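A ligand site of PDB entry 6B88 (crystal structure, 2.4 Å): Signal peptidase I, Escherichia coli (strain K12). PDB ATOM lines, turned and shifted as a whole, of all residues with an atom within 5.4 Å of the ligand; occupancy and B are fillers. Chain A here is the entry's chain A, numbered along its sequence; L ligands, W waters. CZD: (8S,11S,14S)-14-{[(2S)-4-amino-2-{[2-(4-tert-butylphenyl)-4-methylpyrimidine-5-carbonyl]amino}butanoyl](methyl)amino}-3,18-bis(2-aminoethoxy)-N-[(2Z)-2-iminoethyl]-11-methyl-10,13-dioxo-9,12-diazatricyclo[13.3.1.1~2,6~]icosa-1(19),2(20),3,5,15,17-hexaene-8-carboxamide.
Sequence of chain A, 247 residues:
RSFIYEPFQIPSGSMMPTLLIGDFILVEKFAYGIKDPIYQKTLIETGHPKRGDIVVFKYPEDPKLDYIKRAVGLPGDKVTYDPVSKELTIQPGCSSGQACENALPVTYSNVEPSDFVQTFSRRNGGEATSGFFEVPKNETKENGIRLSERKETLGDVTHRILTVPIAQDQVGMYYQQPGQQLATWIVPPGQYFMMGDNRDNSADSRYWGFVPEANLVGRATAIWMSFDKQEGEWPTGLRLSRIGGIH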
ATOM      1  N   GLU A   6       2.573 -15.269  35.259  1.00  0.00           N
ATOM      2  CA  GLU A   6       1.965 -16.138  34.255  1.00  0.00           C
ATOM      3  C   GLU A   6       2.829 -17.359  33.955  1.00  0.00           C
ATOM      4  O   GLU A   6       4.048 -17.228  33.805  1.00  0.00           O
ATOM      5  CB  GLU A   6       1.724 -15.350  32.949  1.00  0.00           C
ATOM      6  CG  GLU A   6       0.572 -15.872  32.098  1.00  0.00           C
ATOM      7  CD  GLU A   6       0.655 -15.505  30.613  1.00  0.00           C
ATOM      8  OE1 GLU A   6       0.908 -14.336  30.281  1.00  0.00           O
ATOM      9  OE2 GLU A   6       0.449 -16.425  29.781  1.00  0.00           O
ATOM     10  N   PRO A   7       2.234 -18.547  33.791  1.00  0.00           N
ATOM     11  CA  PRO A   7       3.043 -19.728  33.472  1.00  0.00           C
ATOM     12  C   PRO A   7       3.266 -19.937  31.972  1.00  0.00           C
ATOM     13  O   PRO A   7       2.378 -19.722  31.140  1.00  0.00           O
ATOM     14  CB  PRO A   7       2.214 -20.882  34.071  1.00  0.00           C
ATOM     15  CG  PRO A   7       0.795 -20.403  34.063  1.00  0.00           C
ATOM     16  CD  PRO A   7       0.802 -18.895  33.947  1.00  0.00           C
ATOM     17  N   PHE A   8       4.484 -20.348  31.639  1.00  0.00           N
ATOM     18  CA  PHE A   8       4.844 -20.657  30.257  1.00  0.00           C
ATOM     19  C   PHE A   8       5.496 -22.033  30.181  1.00  0.00           C
ATOM     20  O   PHE A   8       6.147 -22.485  31.140  1.00  0.00           O
ATOM     21  CB  PHE A   8       5.759 -19.554  29.659  1.00  0.00           C
ATOM     22  CG  PHE A   8       5.016 -18.273  29.331  1.00  0.00           C
ATOM     23  CD1 PHE A   8       4.849 -17.285  30.290  1.00  0.00           C
ATOM     24  CD2 PHE A   8       4.491 -18.072  28.063  1.00  0.00           C
ATOM     25  CE1 PHE A   8       4.161 -16.105  29.988  1.00  0.00           C
ATOM     26  CE2 PHE A   8       3.794 -16.897  27.760  1.00  0.00           C
ATOM     27  CZ  PHE A   8       3.634 -15.921  28.717  1.00  0.00           C
ATOM     28  N   GLN A   9       5.235 -22.724  29.077  1.00  0.00           N
ATOM     29  CA  GLN A   9       5.799 -24.015  28.719  1.00  0.00           C
ATOM     30  C   GLN A   9       7.000 -23.757  27.814  1.00  0.00           C
ATOM     31  O   GLN A   9       6.940 -22.863  26.977  1.00  0.00           O
ATOM     32  CB  GLN A   9       4.743 -24.850  27.974  1.00  0.00           C
ATOM     33  CG  GLN A   9       5.215 -26.192  27.439  1.00  0.00           C
ATOM     34  CD  GLN A   9       4.128 -26.946  26.664  1.00  0.00           C
ATOM     35  OE1 GLN A   9       2.955 -26.611  26.732  1.00  0.00           O
ATOM     36  NE2 GLN A   9       4.554 -27.971  25.957  1.00  0.00           N
ATOM     37  N   ILE A  10       8.086 -24.515  27.992  1.00  0.00           N
ATOM     38  CA  ILE A  10       9.250 -24.358  27.102  1.00  0.00           C
ATOM     39  C   ILE A  10       9.295 -25.557  26.133  1.00  0.00           C
ATOM     40  O   ILE A  10       9.791 -26.631  26.495  1.00  0.00           O
ATOM     41  CB  ILE A  10      10.569 -24.187  27.902  1.00  0.00           C
ATOM     42  CG1 ILE A  10      10.507 -22.959  28.886  1.00  0.00           C
ATOM     43  CG2 ILE A  10      11.802 -24.105  26.971  1.00  0.00           C
ATOM     44  CD1 ILE A  10      10.186 -21.538  28.280  1.00  0.00           C
ATOM     45  N   PRO A  11       8.756 -25.442  24.905  1.00  0.00           N
ATOM     46  CA  PRO A  11       8.767 -26.588  23.978  1.00  0.00           C
ATOM     47  C   PRO A  11       9.973 -26.664  23.047  1.00  0.00           C
ATOM     48  O   PRO A  11      10.098 -27.657  22.312  1.00  0.00           O
ATOM     49  CB  PRO A  11       7.470 -26.365  23.159  1.00  0.00           C
ATOM     50  CG  PRO A  11       7.233 -24.859  23.188  1.00  0.00           C
ATOM     51  CD  PRO A  11       8.081 -24.275  24.316  1.00  0.00           C
ATOM     52  N   SER A  12      10.872 -25.689  23.095  1.00  0.00           N
ATOM     53  CA  SER A  12      12.041 -25.584  22.221  1.00  0.00           C
ATOM     54  C   SER A  12      13.351 -25.602  23.022  1.00  0.00           C
ATOM     55  O   SER A  12      13.367 -25.420  24.247  1.00  0.00           O
ATOM     56  CB  SER A  12      11.974 -24.306  21.372  1.00  0.00           C
ATOM     57  OG  SER A  12      10.848 -24.320  20.530  1.00  0.00           O
ATOM     58  N   SER A  14      16.077 -23.524  22.328  1.00  0.00           N
ATOM     59  CA  SER A  14      16.827 -22.278  22.116  1.00  0.00           C
ATOM     60  C   SER A  14      17.459 -21.705  23.392  1.00  0.00           C
ATOM     61  O   SER A  14      18.432 -20.956  23.276  1.00  0.00           O
ATOM     62  CB  SER A  14      15.888 -21.226  21.472  1.00  0.00           C
ATOM     63  OG  SER A  14      15.145 -20.479  22.414  1.00  0.00           O
ATOM     64  N   PHE A  24       8.656 -25.727  32.829  1.00  0.00           N
ATOM     65  CA  PHE A  24       7.493 -24.860  33.041  1.00  0.00           C
ATOM     66  C   PHE A  24       7.964 -23.729  33.950  1.00  0.00           C
ATOM     67  O   PHE A  24       8.401 -23.977  35.100  1.00  0.00           O
ATOM     68  CB  PHE A  24       6.310 -25.657  33.566  1.00  0.00           C
ATOM     69  CG  PHE A  24       5.674 -26.528  32.504  1.00  0.00           C
ATOM     70  CD1 PHE A  24       6.241 -27.747  32.169  1.00  0.00           C
ATOM     71  CD2 PHE A  24       4.562 -26.101  31.807  1.00  0.00           C
ATOM     72  CE1 PHE A  24       5.698 -28.529  31.168  1.00  0.00           C
ATOM     73  CE2 PHE A  24       4.013 -26.892  30.797  1.00  0.00           C
ATOM     74  CZ  PHE A  24       4.578 -28.110  30.484  1.00  0.00           C
ATOM     75  N   VAL A  56      10.309 -12.829  28.188  1.00  0.00           N
ATOM     76  CA  VAL A  56       9.238 -13.305  27.310  1.00  0.00           C
ATOM     77  C   VAL A  56       8.632 -12.077  26.610  1.00  0.00           C
ATOM     78  O   VAL A  56       8.472 -11.023  27.251  1.00  0.00           O
ATOM     79  CB  VAL A  56       8.182 -14.112  28.105  1.00  0.00           C
ATOM     80  CG1 VAL A  56       6.921 -14.403  27.282  1.00  0.00           C
ATOM     81  CG2 VAL A  56       8.766 -15.466  28.588  1.00  0.00           C
ATOM     82  N   LEU A  65       2.284 -14.827  18.807  1.00  0.00           N
ATOM     83  CA  LEU A  65       3.180 -15.798  19.428  1.00  0.00           C
ATOM     84  C   LEU A  65       4.083 -15.132  20.464  1.00  0.00           C
ATOM     85  O   LEU A  65       4.578 -14.026  20.248  1.00  0.00           O
ATOM     86  CB  LEU A  65       4.036 -16.454  18.351  1.00  0.00           C
ATOM     87  CG  LEU A  65       3.634 -17.740  17.622  1.00  0.00           C
ATOM     88  CD1 LEU A  65       2.141 -17.839  17.337  1.00  0.00           C
ATOM     89  CD2 LEU A  65       4.402 -17.868  16.307  1.00  0.00           C
ATOM     90  N   ASP A  66       4.354 -15.839  21.585  1.00  0.00           N
ATOM     91  CA  ASP A  66       5.313 -15.412  22.600  1.00  0.00           C
ATOM     92  C   ASP A  66       6.622 -16.172  22.401  1.00  0.00           C
ATOM     93  O   ASP A  66       6.619 -17.365  22.103  1.00  0.00           O
ATOM     94  CB  ASP A  66       4.809 -15.694  24.030  1.00  0.00           C
ATOM     95  CG  ASP A  66       3.565 -14.898  24.403  1.00  0.00           C
ATOM     96  OD1 ASP A  66       2.532 -15.547  24.682  1.00  0.00           O
ATOM     97  OD2 ASP A  66       3.630 -13.666  24.454  1.00  0.00           O
ATOM     98  N   TYR A  67       7.753 -15.469  22.575  1.00  0.00           N
ATOM     99  CA  TYR A  67       9.081 -16.048  22.432  1.00  0.00           C
ATOM    100  C   TYR A  67       9.864 -15.743  23.692  1.00  0.00           C
ATOM    101  O   TYR A  67       9.598 -14.756  24.386  1.00  0.00           O
ATOM    102  CB  TYR A  67       9.817 -15.461  21.232  1.00  0.00           C
ATOM    103  CG  TYR A  67       9.666 -16.186  19.914  1.00  0.00           C
ATOM    104  CD1 TYR A  67       8.423 -16.301  19.306  1.00  0.00           C
ATOM    105  CD2 TYR A  67      10.773 -16.685  19.236  1.00  0.00           C
ATOM    106  CE1 TYR A  67       8.283 -16.938  18.066  1.00  0.00           C
ATOM    107  CE2 TYR A  67      10.634 -17.324  18.010  1.00  0.00           C
ATOM    108  CZ  TYR A  67       9.388 -17.439  17.424  1.00  0.00           C
ATOM    109  OH  TYR A  67       9.255 -18.070  16.207  1.00  0.00           O
ATOM    110  N   ILE A  68      10.859 -16.589  24.012  1.00  0.00           N
ATOM    111  CA  ILE A  68      11.700 -16.372  25.186  1.00  0.00           C
ATOM    112  C   ILE A  68      13.164 -16.382  24.763  1.00  0.00           C
ATOM    113  O   ILE A  68      13.632 -17.346  24.113  1.00  0.00           O
ATOM    114  CB  ILE A  68      11.394 -17.384  26.311  1.00  0.00           C
ATOM    115  CG1 ILE A  68      12.235 -17.075  27.556  1.00  0.00           C
ATOM    116  CG2 ILE A  68      11.497 -18.864  25.870  1.00  0.00           C
ATOM    117  CD1 ILE A  68      11.706 -17.636  28.835  1.00  0.00           C
ATOM    118  N   LYS A  69      13.901 -15.318  25.119  1.00  0.00           N
ATOM    119  CA  LYS A  69      15.343 -15.193  24.845  1.00  0.00           C
ATOM    120  C   LYS A  69      15.970 -14.380  25.981  1.00  0.00           C
ATOM    121  O   LYS A  69      15.281 -13.937  26.924  1.00  0.00           O
ATOM    122  CB  LYS A  69      15.616 -14.511  23.485  1.00  0.00           C
ATOM    123  CG  LYS A  69      15.061 -15.177  22.192  1.00  0.00           C
ATOM    124  CD  LYS A  69      15.347 -16.665  22.043  1.00  0.00           C
ATOM    125  CE  LYS A  69      14.833 -17.215  20.718  1.00  0.00           C
ATOM    126  NZ  LYS A  69      13.753 -18.264  20.709  1.00  0.00           N
ATOM    127  N   SER A 202      19.109 -21.251  17.866  1.00  0.00           N
ATOM    128  CA  SER A 202      18.211 -20.186  18.342  1.00  0.00           C
ATOM    129  C   SER A 202      17.896 -19.158  17.239  1.00  0.00           C
ATOM    130  O   SER A 202      18.780 -18.434  16.778  1.00  0.00           O
ATOM    131  CB  SER A 202      18.823 -19.484  19.554  1.00  0.00           C
ATOM    132  OG  SER A 202      17.970 -18.460  20.034  1.00  0.00           O
ATOM    133  N   ALA A 203      16.614 -19.064  16.876  1.00  0.00           N
ATOM    134  CA  ALA A 203      16.124 -18.060  15.932  1.00  0.00           C
ATOM    135  C   ALA A 203      15.872 -16.787  16.721  1.00  0.00           C
ATOM    136  O   ALA A 203      14.795 -16.612  17.293  1.00  0.00           O
ATOM    137  CB  ALA A 203      14.851 -18.558  15.236  1.00  0.00           C
ATOM    138  N   TRP A 224       8.745 -23.838  37.984  1.00  0.00           N
ATOM    139  CA  TRP A 224       7.849 -24.375  39.010  1.00  0.00           C
ATOM    140  C   TRP A 224       7.509 -25.848  38.810  1.00  0.00           C
ATOM    141  O   TRP A 224       6.961 -26.473  39.733  1.00  0.00           O
ATOM    142  CB  TRP A 224       6.564 -23.510  39.081  1.00  0.00           C
ATOM    143  CG  TRP A 224       5.722 -23.511  37.841  1.00  0.00           C
ATOM    144  CD1 TRP A 224       5.819 -22.668  36.770  1.00  0.00           C
ATOM    145  CD2 TRP A 224       4.630 -24.403  37.543  1.00  0.00           C
ATOM    146  NE1 TRP A 224       4.869 -22.979  35.818  1.00  0.00           N
ATOM    147  CE2 TRP A 224       4.124 -24.033  36.278  1.00  0.00           C
ATOM    148  CE3 TRP A 224       4.039 -25.462  38.222  1.00  0.00           C
ATOM    149  CZ2 TRP A 224       3.057 -24.708  35.673  1.00  0.00           C
ATOM    150  CZ3 TRP A 224       2.980 -26.137  37.632  1.00  0.00           C
ATOM    151  CH2 TRP A 224       2.501 -25.752  36.369  1.00  0.00           C
HETATM  152  C4  CZD L   1      -1.020 -23.112  32.660  1.00  0.00           C
HETATM  153  C14 CZD L   1      -2.707 -23.434  38.951  1.00  0.00           C
HETATM  154  C5  CZD L   1      -1.361 -23.511  34.037  1.00  0.00           C
HETATM  155  C6  CZD L   1      -2.663 -23.369  34.514  1.00  0.00           C
HETATM  156  C11 CZD L   1      -2.425 -24.664  38.092  1.00  0.00           C
HETATM  157  C7  CZD L   1      -2.993 -23.732  35.804  1.00  0.00           C
HETATM  158  C8  CZD L   1      -2.033 -24.264  36.663  1.00  0.00           C
HETATM  159  C9  CZD L   1      -0.735 -24.402  36.194  1.00  0.00           C
HETATM  160  C10 CZD L   1      -0.397 -24.034  34.905  1.00  0.00           C
HETATM  161  C12 CZD L   1      -3.697 -25.512  38.070  1.00  0.00           C
HETATM  162  C13 CZD L   1      -1.316 -25.468  38.745  1.00  0.00           C
HETATM  163  N1  CZD L   1       0.251 -23.279  32.280  1.00  0.00           N
HETATM  164  N2  CZD L   1       0.787 -20.984  28.592  1.00  0.00           N
HETATM  165  C3  CZD L   1      -1.687 -22.263  30.676  1.00  0.00           C
HETATM  166  N3  CZD L   1      -0.472 -17.185  26.255  1.00  0.00           N
HETATM  167  N   CZD L   1      -2.014 -22.621  31.917  1.00  0.00           N
HETATM  168  C   CZD L   1       1.998 -23.122  30.639  1.00  0.00           C
HETATM  169  O   CZD L   1      -0.589 -22.575  27.806  1.00  0.00           O
HETATM  170  C1  CZD L   1       0.570 -22.923  31.024  1.00  0.00           C
HETATM  171  C15 CZD L   1      -0.074 -21.983  28.763  1.00  0.00           C
HETATM  172  C16 CZD L   1       1.087 -20.557  27.244  1.00  0.00           C
HETATM  173  C17 CZD L   1       0.803 -19.076  27.087  1.00  0.00           C
HETATM  174  C18 CZD L   1      -0.579 -18.515  26.836  1.00  0.00           C
HETATM  175  C19 CZD L   1       2.477 -21.029  26.819  1.00  0.00           C
HETATM  176  C2  CZD L   1      -0.414 -22.386  30.153  1.00  0.00           C
HETATM  177  C20 CZD L   1       1.723 -21.025  24.453  1.00  0.00           C
HETATM  178  C21 CZD L   1       4.039 -21.670  25.152  1.00  0.00           C
HETATM  179  C22 CZD L   1       4.092 -22.548  23.923  1.00  0.00           C
HETATM  180  C23 CZD L   1       3.626 -23.854  23.932  1.00  0.00           C
HETATM  181  C24 CZD L   1       3.687 -24.641  22.789  1.00  0.00           C
HETATM  182  C25 CZD L   1       4.233 -24.091  21.630  1.00  0.00           C
HETATM  183  C26 CZD L   1       4.702 -22.787  21.599  1.00  0.00           C
HETATM  184  C27 CZD L   1       4.628 -22.021  22.759  1.00  0.00           C
HETATM  185  C28 CZD L   1       5.302 -22.124  20.414  1.00  0.00           C
HETATM  186  C29 CZD L   1       6.469 -21.415  20.646  1.00  0.00           C
HETATM  187  C30 CZD L   1       7.131 -20.749  19.627  1.00  0.00           C
HETATM  188  C31 CZD L   1       6.603 -20.808  18.350  1.00  0.00           C
HETATM  189  C32 CZD L   1       5.443 -21.503  18.078  1.00  0.00           C
HETATM  190  C33 CZD L   1       4.796 -22.158  19.121  1.00  0.00           C
HETATM  191  C34 CZD L   1       3.055 -22.854  17.652  1.00  0.00           C
HETATM  192  C35 CZD L   1       1.815 -23.726  17.798  1.00  0.00           C
HETATM  193  C36 CZD L   1       8.395 -19.999  19.924  1.00  0.00           C
HETATM  194  C37 CZD L   1       8.865 -20.275  21.364  1.00  0.00           C
HETATM  195  C38 CZD L   1       7.863 -20.219  23.570  1.00  0.00           C
HETATM  196  C39 CZD L   1       6.996 -19.444  24.544  1.00  0.00           C
HETATM  197  C40 CZD L   1       4.795 -20.358  24.860  1.00  0.00           C
HETATM  198  C41 CZD L   1       7.881 -18.767  25.590  1.00  0.00           C
HETATM  199  C42 CZD L   1      10.279 -19.753  21.553  1.00  0.00           C
HETATM  200  C45 CZD L   1       3.938 -26.154  20.500  1.00  0.00           C
HETATM  201  C46 CZD L   1       4.153 -26.671  19.074  1.00  0.00           C
HETATM  202  N10 CZD L   1       5.445 -27.315  18.975  1.00  0.00           N
HETATM  203  N4  CZD L   1       2.706 -21.222  25.504  1.00  0.00           N
HETATM  204  N5  CZD L   1       0.646 -23.028  17.296  1.00  0.00           N
HETATM  205  N6  CZD L   1       7.942 -19.706  22.329  1.00  0.00           N
HETATM  206  N7  CZD L   1       6.086 -20.380  25.188  1.00  0.00           N
HETATM  207  O1  CZD L   1       3.335 -21.213  27.659  1.00  0.00           O
HETATM  208  O2  CZD L   1       3.648 -22.871  18.945  1.00  0.00           O
HETATM  209  O3  CZD L   1       8.443 -21.254  23.909  1.00  0.00           O
HETATM  210  O4  CZD L   1       4.218 -19.382  24.362  1.00  0.00           O
HETATM  211  O5  CZD L   1      10.524 -18.860  22.378  1.00  0.00           O
HETATM  212  O6  CZD L   1       4.339 -24.789  20.470  1.00  0.00           O
HETATM  213  C43 CZD L   1      12.617 -19.993  21.045  1.00  0.00           C
HETATM  214  C44 CZD L   1      13.126 -19.369  19.832  1.00  0.00           C
HETATM  215  N8  CZD L   1      11.227 -20.300  20.789  1.00  0.00           N
HETATM  216  N9  CZD L   1      13.138 -19.473  18.697  1.00  0.00           N
HETATM  217  O   HOH W   1       1.240 -20.774  14.751  1.00  0.00           O
HETATM  218  O   HOH W   2       6.017 -24.460  16.490  1.00  0.00           O
HETATM  219  O   HOH W   3       2.568 -17.933  22.633  1.00  0.00           O
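The side-chain amino group (NZ) of Lys 69 is covalently linked to a carbon (C44) of the ligand, at 1.5 Å. O of Asp 66 sits at hydrogen-bond distance from N6 of the ligand, at 2.7 Å. The side-chain carboxylate (OD1) of Asp 66 lies within salt-bridge range of a nitrogen (N3) of the ligand (3.8 Å). N of Gln 9 sits at hydrogen-bond distance from O1 of the ligand (2.8 Å). The backbone carbonyl oxygen (O) of Gln 9 lies within hydrogen-bond range of a nitrogen (N7) of the ligand (3.2 Å). An oxygen (O5) of the ligand lies within hydrogen-bond range of the backbone NH of Ile 68. The backbone carbonyl oxygen of Pro 7 lies within hydrogen-bond range of a nitrogen (N2) of the ligand, at 3.3 Å. The side-chain carboxylate of Glu 6 lies within salt-bridge range of a nitrogen (N3) of the ligand (3.7 Å).
The side-chain amino group (NZ) of Lys 69 is in hydrogen-bond range of the side-chain hydroxyl (OG) of Ser 14 (3.1 Å). N of Trp 224 sits at hydrogen-bond distance from O of Phe 24 (2.9 Å).
Merely in contact with the ligand: Ser 14 (2.9 Å), Phe 8 (3.1 Å), Pro 11 (3.1 Å), Tyr 67 (3.2 Å), Trp 224 (3.5 Å) and Ala 203 (3.6 Å). 12 residues have an atom within 4 Å of the ligand: Glu 6, Pro 7, Phe 8, Gln 9, Pro 11, Ser 14, Asp 66, Tyr 67, Ile 68, Lys 69, Ala 203 and Trp 224.
Water W3 bridges an oxygen (O4) of the ligand (2.8 Å) and the backbone NH (N) of Asp 66 (2.9 Å).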
